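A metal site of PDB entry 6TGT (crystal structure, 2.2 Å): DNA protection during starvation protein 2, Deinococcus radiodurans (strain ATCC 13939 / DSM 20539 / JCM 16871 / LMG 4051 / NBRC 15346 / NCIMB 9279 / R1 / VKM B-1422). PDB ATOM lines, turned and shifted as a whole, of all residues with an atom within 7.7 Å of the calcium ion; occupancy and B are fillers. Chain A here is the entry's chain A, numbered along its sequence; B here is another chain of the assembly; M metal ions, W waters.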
ATOM      1  N   PHE A 186      14.793 -21.140  14.598  1.00  0.00           N
ATOM      2  CA  PHE A 186      14.560 -22.337  15.393  1.00  0.00           C
ATOM      3  C   PHE A 186      15.521 -22.413  16.575  1.00  0.00           C
ATOM      4  O   PHE A 186      15.164 -22.964  17.624  1.00  0.00           O
ATOM      5  CB  PHE A 186      14.690 -23.585  14.532  1.00  0.00           C
ATOM      6  CG  PHE A 186      13.509 -23.829  13.633  1.00  0.00           C
ATOM      7  CD1 PHE A 186      12.321 -24.336  14.145  1.00  0.00           C
ATOM      8  CD2 PHE A 186      13.586 -23.569  12.276  1.00  0.00           C
ATOM      9  CE1 PHE A 186      11.234 -24.558  13.323  1.00  0.00           C
ATOM     10  CE2 PHE A 186      12.499 -23.790  11.439  1.00  0.00           C
ATOM     11  CZ  PHE A 186      11.326 -24.290  11.966  1.00  0.00           C
ATOM     12  N   GLN A 188      17.293 -19.513  17.740  1.00  0.00           N
ATOM     13  CA  GLN A 188      17.636 -18.146  18.095  1.00  0.00           C
ATOM     14  C   GLN A 188      17.587 -17.962  19.608  1.00  0.00           C
ATOM     15  O   GLN A 188      16.602 -18.316  20.262  1.00  0.00           O
ATOM     16  CB  GLN A 188      16.687 -17.169  17.406  1.00  0.00           C
ATOM     17  CG  GLN A 188      16.810 -15.736  17.912  1.00  0.00           C
ATOM     18  CD  GLN A 188      18.169 -15.137  17.615  1.00  0.00           C
ATOM     19  OE1 GLN A 188      18.569 -15.003  16.453  1.00  0.00           O
ATOM     20  NE2 GLN A 188      18.892 -14.765  18.667  1.00  0.00           N
ATOM     21  N   THR A 190      17.194 -16.213  23.176  1.00  0.00           N
ATOM     22  CA  THR A 190      16.272 -15.248  23.758  1.00  0.00           C
ATOM     23  C   THR A 190      16.686 -14.975  25.190  1.00  0.00           C
ATOM     24  O   THR A 190      17.430 -15.756  25.792  1.00  0.00           O
ATOM     25  CB  THR A 190      14.823 -15.763  23.711  1.00  0.00           C
ATOM     26  OG1 THR A 190      14.725 -16.972  24.471  1.00  0.00           O
ATOM     27  CG2 THR A 190      14.393 -16.020  22.274  1.00  0.00           C
ATOM     28  N   THR A 192      14.990 -15.296  27.889  1.00  0.00           N
ATOM     29  CA  THR A 192      14.455 -16.308  28.793  1.00  0.00           C
ATOM     30  C   THR A 192      14.822 -17.725  28.382  1.00  0.00           C
ATOM     31  O   THR A 192      14.515 -18.666  29.134  1.00  0.00           O
ATOM     32  CB  THR A 192      12.926 -16.194  28.862  1.00  0.00           C
ATOM     33  OG1 THR A 192      12.342 -16.745  27.687  1.00  0.00           O
ATOM     34  CG2 THR A 192      12.508 -14.739  29.002  1.00  0.00           C
ATOM     35  N   ASP A 193      15.484 -17.916  27.233  1.00  0.00           N
ATOM     36  CA  ASP A 193      15.795 -19.246  26.740  1.00  0.00           C
ATOM     37  C   ASP A 193      16.873 -19.167  25.671  1.00  0.00           C
ATOM     38  O   ASP A 193      16.690 -18.479  24.659  1.00  0.00           O
ATOM     39  CB  ASP A 193      14.538 -19.918  26.186  1.00  0.00           C
ATOM     40  CG  ASP A 193      14.698 -21.421  25.996  1.00  0.00           C
ATOM     41  OD1 ASP A 193      15.838 -21.914  25.970  1.00  0.00           O
ATOM     42  OD2 ASP A 193      13.658 -22.111  25.879  1.00  0.00           O
ATOM     43  N   PRO A 194      18.009 -19.853  25.847  1.00  0.00           N
ATOM     44  CA  PRO A 194      19.028 -19.856  24.787  1.00  0.00           C
ATOM     45  C   PRO A 194      18.613 -20.629  23.548  1.00  0.00           C
ATOM     46  O   PRO A 194      19.222 -20.420  22.490  1.00  0.00           O
ATOM     47  CB  PRO A 194      20.238 -20.500  25.469  1.00  0.00           C
ATOM     48  CG  PRO A 194      19.658 -21.312  26.587  1.00  0.00           C
ATOM     49  CD  PRO A 194      18.457 -20.554  27.061  1.00  0.00           C
ATOM     50  N   ASN A 195      17.618 -21.505  23.646  1.00  0.00           N
ATOM     51  CA  ASN A 195      17.142 -22.313  22.526  1.00  0.00           C
ATOM     52  C   ASN A 195      18.283 -23.126  21.907  1.00  0.00           C
ATOM     53  O   ASN A 195      18.650 -22.969  20.741  1.00  0.00           O
ATOM     54  CB  ASN A 195      16.451 -21.449  21.467  1.00  0.00           C
ATOM     55  CG  ASN A 195      15.078 -20.969  21.921  1.00  0.00           C
ATOM     56  OD1 ASN A 195      14.339 -21.704  22.584  1.00  0.00           O
ATOM     57  ND2 ASN A 195      14.736 -19.738  21.573  1.00  0.00           N
ATOM     58  N   THR A 196      18.860 -24.004  22.735  1.00  0.00           N
ATOM     59  CA  THR A 196      19.969 -24.847  22.285  1.00  0.00           C
ATOM     60  C   THR A 196      19.518 -25.980  21.374  1.00  0.00           C
ATOM     61  O   THR A 196      20.378 -26.641  20.775  1.00  0.00           O
ATOM     62  CB  THR A 196      20.705 -25.423  23.492  1.00  0.00           C
ATOM     63  OG1 THR A 196      19.937 -26.496  24.065  1.00  0.00           O
ATOM     64  CG2 THR A 196      20.939 -24.357  24.547  1.00  0.00           C
ATOM     65  N   PHE A 198      18.095 -28.765  22.347  1.00  0.00           N
ATOM     66  CA  PHE A 198      18.286 -30.068  22.986  1.00  0.00           C
ATOM     67  C   PHE A 198      17.057 -30.948  22.830  1.00  0.00           C
ATOM     68  O   PHE A 198      17.176 -32.177  22.768  1.00  0.00           O
ATOM     69  CB  PHE A 198      18.622 -29.879  24.463  1.00  0.00           C
ATOM     70  CG  PHE A 198      17.434 -29.579  25.332  1.00  0.00           C
ATOM     71  CD1 PHE A 198      16.893 -28.302  25.367  1.00  0.00           C
ATOM     72  CD2 PHE A 198      16.854 -30.567  26.105  1.00  0.00           C
ATOM     73  CE1 PHE A 198      15.790 -28.020  26.159  1.00  0.00           C
ATOM     74  CE2 PHE A 198      15.748 -30.291  26.890  1.00  0.00           C
ATOM     75  CZ  PHE A 198      15.225 -29.022  26.923  1.00  0.00           C
ATOM     76  N   ASP A 199      15.861 -30.345  22.769  1.00  0.00           N
ATOM     77  CA  ASP A 199      14.638 -31.123  22.666  1.00  0.00           C
ATOM     78  C   ASP A 199      14.493 -31.816  21.316  1.00  0.00           C
ATOM     79  O   ASP A 199      13.781 -32.831  21.225  1.00  0.00           O
ATOM     80  CB  ASP A 199      13.423 -30.231  22.912  1.00  0.00           C
ATOM     81  CG  ASP A 199      13.439 -28.969  22.068  1.00  0.00           C
ATOM     82  OD1 ASP A 199      14.535 -28.369  21.911  1.00  0.00           O
ATOM     83  OD2 ASP A 199      12.369 -28.584  21.561  1.00  0.00           O
ATOM     84  N   SER B  74      10.933 -17.095  18.637  1.00  0.00           N
ATOM     85  CA  SER B  74      12.094 -17.942  18.420  1.00  0.00           C
ATOM     86  C   SER B  74      11.919 -19.248  19.180  1.00  0.00           C
ATOM     87  O   SER B  74      11.123 -19.338  20.122  1.00  0.00           O
ATOM     88  CB  SER B  74      13.386 -17.245  18.861  1.00  0.00           C
ATOM     89  OG  SER B  74      13.511 -15.960  18.271  1.00  0.00           O
ATOM     90  N   GLY B  75      12.676 -20.244  18.772  1.00  0.00           N
ATOM     91  CA  GLY B  75      12.678 -21.532  19.442  1.00  0.00           C
ATOM     92  C   GLY B  75      12.113 -22.630  18.554  1.00  0.00           C
ATOM     93  O   GLY B  75      11.926 -22.471  17.347  1.00  0.00           O
ATOM     94  N   THR B  76      11.829 -23.768  19.207  1.00  0.00           N
ATOM     95  CA  THR B  76      11.314 -24.933  18.481  1.00  0.00           C
ATOM     96  C   THR B  76       9.976 -24.646  17.819  1.00  0.00           C
ATOM     97  O   THR B  76       9.733 -25.061  16.686  1.00  0.00           O
ATOM     98  CB  THR B  76      11.200 -26.120  19.443  1.00  0.00           C
ATOM     99  OG1 THR B  76      12.484 -26.449  19.961  1.00  0.00           O
ATOM    100  CG2 THR B  76      10.619 -27.333  18.729  1.00  0.00           C
ATOM    101  N   LEU B  77       9.104 -23.908  18.512  1.00  0.00           N
ATOM    102  CA  LEU B  77       7.758 -23.623  18.013  1.00  0.00           C
ATOM    103  C   LEU B  77       7.657 -22.245  17.371  1.00  0.00           C
ATOM    104  O   LEU B  77       6.557 -21.692  17.294  1.00  0.00           O
ATOM    105  CB  LEU B  77       6.744 -23.745  19.154  1.00  0.00           C
ATOM    106  CG  LEU B  77       6.399 -25.153  19.627  1.00  0.00           C
ATOM    107  CD1 LEU B  77       5.410 -25.101  20.783  1.00  0.00           C
ATOM    108  CD2 LEU B  77       5.835 -25.981  18.481  1.00  0.00           C
ATOM    109  N   LEU B 131      11.798 -12.975  21.113  1.00  0.00           N
ATOM    110  CA  LEU B 131      10.873 -13.591  22.058  1.00  0.00           C
ATOM    111  C   LEU B 131      10.939 -15.096  21.949  1.00  0.00           C
ATOM    112  O   LEU B 131      10.986 -15.655  20.840  1.00  0.00           O
ATOM    113  CB  LEU B 131       9.438 -13.112  21.810  1.00  0.00           C
ATOM    114  CG  LEU B 131       9.123 -11.669  22.179  1.00  0.00           C
ATOM    115  CD1 LEU B 131       7.713 -11.321  21.754  1.00  0.00           C
ATOM    116  CD2 LEU B 131       9.301 -11.440  23.666  1.00  0.00           C
ATOM    117  N   ASP B 132      10.953 -15.771  23.091  1.00  0.00           N
ATOM    118  CA  ASP B 132      10.954 -17.225  23.104  1.00  0.00           C
ATOM    119  C   ASP B 132       9.549 -17.753  22.877  1.00  0.00           C
ATOM    120  O   ASP B 132       8.548 -17.106  23.203  1.00  0.00           O
ATOM    121  CB  ASP B 132      11.492 -17.750  24.438  1.00  0.00           C
ATOM    122  CG  ASP B 132      11.814 -19.237  24.377  1.00  0.00           C
ATOM    123  OD1 ASP B 132      12.623 -19.619  23.509  1.00  0.00           O
ATOM    124  OD2 ASP B 132      11.263 -20.000  25.193  1.00  0.00           O
ATOM    125  N   ASP B 133       9.471 -18.951  22.292  1.00  0.00           N
ATOM    126  CA  ASP B 133       8.178 -19.557  21.995  1.00  0.00           C
ATOM    127  C   ASP B 133       7.386 -19.823  23.268  1.00  0.00           C
ATOM    128  O   ASP B 133       6.177 -19.559  23.324  1.00  0.00           O
ATOM    129  CB  ASP B 133       8.362 -20.843  21.192  1.00  0.00           C
ATOM    130  CG  ASP B 133       9.375 -21.790  21.831  1.00  0.00           C
ATOM    131  OD1 ASP B 133       9.942 -21.425  22.889  1.00  0.00           O
ATOM    132  OD2 ASP B 133       9.593 -22.877  21.274  1.00  0.00           O
ATOM    133  N   ALA B 134       8.047 -20.335  24.299  1.00  0.00           N
ATOM    134  CA  ALA B 134       7.369 -20.568  25.578  1.00  0.00           C
ATOM    135  C   ALA B 134       6.916 -19.262  26.217  1.00  0.00           C
ATOM    136  O   ALA B 134       5.859 -19.216  26.863  1.00  0.00           O
ATOM    137  CB  ALA B 134       8.278 -21.344  26.530  1.00  0.00           C
ATOM    138  N   GLN B 135       7.695 -18.194  26.040  1.00  0.00           N
ATOM    139  CA  GLN B 135       7.298 -16.889  26.563  1.00  0.00           C
ATOM    140  C   GLN B 135       6.080 -16.346  25.814  1.00  0.00           C
ATOM    141  O   GLN B 135       5.189 -15.758  26.429  1.00  0.00           O
ATOM    142  CB  GLN B 135       8.473 -15.909  26.468  1.00  0.00           C
ATOM    143  CG  GLN B 135       8.217 -14.564  27.137  1.00  0.00           C
ATOM    144  CD  GLN B 135       9.356 -13.587  26.901  1.00  0.00           C
ATOM    145  OE1 GLN B 135      10.179 -13.787  26.008  1.00  0.00           O
ATOM    146  NE2 GLN B 135       9.393 -12.519  27.695  1.00  0.00           N
ATOM    147  N   GLY B 197       5.964 -28.191  29.358  1.00  0.00           N
ATOM    148  CA  GLY B 197       6.689 -27.300  28.477  1.00  0.00           C
ATOM    149  C   GLY B 197       8.180 -27.264  28.709  1.00  0.00           C
ATOM    150  O   GLY B 197       8.835 -26.300  28.293  1.00  0.00           O
ATOM    151  N   PHE B 198       8.742 -28.286  29.360  1.00  0.00           N
ATOM    152  CA  PHE B 198      10.181 -28.299  29.625  1.00  0.00           C
ATOM    153  C   PHE B 198      10.983 -28.348  28.335  1.00  0.00           C
ATOM    154  O   PHE B 198      12.099 -27.820  28.276  1.00  0.00           O
ATOM    155  CB  PHE B 198      10.534 -29.485  30.517  1.00  0.00           C
ATOM    156  CG  PHE B 198      10.613 -30.799  29.794  1.00  0.00           C
ATOM    157  CD1 PHE B 198       9.455 -31.488  29.462  1.00  0.00           C
ATOM    158  CD2 PHE B 198      11.834 -31.342  29.440  1.00  0.00           C
ATOM    159  CE1 PHE B 198       9.519 -32.697  28.785  1.00  0.00           C
ATOM    160  CE2 PHE B 198      11.900 -32.544  28.757  1.00  0.00           C
ATOM    161  CZ  PHE B 198      10.749 -33.222  28.440  1.00  0.00           C
ATOM    162  N   ASP B 199      10.438 -28.982  27.285  1.00  0.00           N
ATOM    163  CA  ASP B 199      11.164 -29.108  26.033  1.00  0.00           C
ATOM    164  C   ASP B 199      11.319 -27.779  25.305  1.00  0.00           C
ATOM    165  O   ASP B 199      12.253 -27.631  24.498  1.00  0.00           O
ATOM    166  CB  ASP B 199      10.464 -30.110  25.118  1.00  0.00           C
ATOM    167  CG  ASP B 199       8.981 -29.827  24.959  1.00  0.00           C
ATOM    168  OD1 ASP B 199       8.330 -29.467  25.975  1.00  0.00           O
ATOM    169  OD2 ASP B 199       8.472 -29.956  23.830  1.00  0.00           O
ATOM    170  N   ILE B 200      10.451 -26.806  25.565  1.00  0.00           N
ATOM    171  CA  ILE B 200      10.497 -25.509  24.895  1.00  0.00           C
ATOM    172  C   ILE B 200      10.986 -24.420  25.835  1.00  0.00           C
ATOM    173  O   ILE B 200      10.931 -23.234  25.478  1.00  0.00           O
ATOM    174  CB  ILE B 200       9.133 -25.145  24.291  1.00  0.00           C
ATOM    175  CG1 ILE B 200       8.061 -25.118  25.370  1.00  0.00           C
ATOM    176  CG2 ILE B 200       8.769 -26.123  23.186  1.00  0.00           C
ATOM    177  CD1 ILE B 200       6.739 -24.519  24.916  1.00  0.00           C
ATOM    178  N   ASN B 201      11.462 -24.765  27.032  1.00  0.00           N
ATOM    179  CA  ASN B 201      11.878 -23.770  28.009  1.00  0.00           C
ATOM    180  C   ASN B 201      13.167 -24.193  28.703  1.00  0.00           C
ATOM    181  O   ASN B 201      13.300 -24.086  29.931  1.00  0.00           O
ATOM    182  CB  ASN B 201      10.757 -23.521  29.034  1.00  0.00           C
ATOM    183  CG  ASN B 201      10.966 -22.243  29.820  1.00  0.00           C
ATOM    184  OD1 ASN B 201      11.490 -21.257  29.298  1.00  0.00           O
ATOM    185  ND2 ASN B 201      10.544 -22.250  31.081  1.00  0.00           N
ATOM    186  N   ASN B 202      14.144 -24.580  27.898  1.00  0.00           N
ATOM    187  CA  ASN B 202      15.503 -24.956  28.379  1.00  0.00           C
ATOM    188  C   ASN B 202      15.464 -25.966  29.533  1.00  0.00           C
ATOM    189  O   ASN B 202      16.245 -25.806  30.455  1.00  0.00           O
ATOM    190  CB  ASN B 202      16.292 -23.714  28.810  1.00  0.00           C
ATOM    191  CG  ASN B 202      17.779 -23.931  28.797  1.00  0.00           C
ATOM    192  OD1 ASN B 202      18.269 -24.805  28.107  1.00  0.00           O
ATOM    193  ND2 ASN B 202      18.515 -23.161  29.567  1.00  0.00           N
HETATM  194 CA    CA M   1      12.247 -21.938  23.822  1.00  0.00          CA
HETATM  195  O   HOH W   1      12.011 -23.791  22.184  1.00  0.00           O
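OD2 of Asp 133 of chain B lies within hydrogen-bond range of N of Thr 76 of chain B, at 3.2 Å.
The backbone NH (N) of Asp 133 of chain B lies within hydrogen-bond range of the backbone carbonyl oxygen (O) of Ser 74 of chain B (2.8 Å).
O of Asp 193 is in hydrogen-bond range of OG1 of Thr 190, at 2.5 Å.
The backbone NH (N) of Ala 134 of chain B lies close to the side-chain carboxylate (OD2) of Asp 132 of chain B, at 3.4 Å.
The side-chain carboxylate (OD2) of Asp 193 sits close to the backbone NH (N) of Asn 202 of chain B (3.2 Å).
The side-chain carboxylate (OD2) of Asp 133 of chain B lies within hydrogen-bond range of the backbone NH (N) of Leu 77 of chain B, at 3.0 Å.
ND2 of Asn 195 sits at hydrogen-bond distance from O of Gln 188 (2.7 Å).
OD1 of Asp 132 of chain B binds the calcium ion.
The side-chain amide oxygen (OD1) of Asn 195 binds the calcium ion (2.4 Å).
O of Ile 200 of chain B binds the calcium ion (2.5 Å).
Water W1 is bound to the calcium ion (2.5 Å).
OD2 of Asp 193 is bound to the calcium ion (2.5 Å).
The side-chain carboxylate (OD1) of Asp 133 of chain B is bound to the calcium ion (2.5 Å).
OD2 of Asp 132 of chain B binds the calcium ion (2.6 Å).
Water W1 lies within hydrogen-bond range of OD2 of Asp 133 of chain B (2.7 Å) and N of Thr 76 of chain B (3.0 Å).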
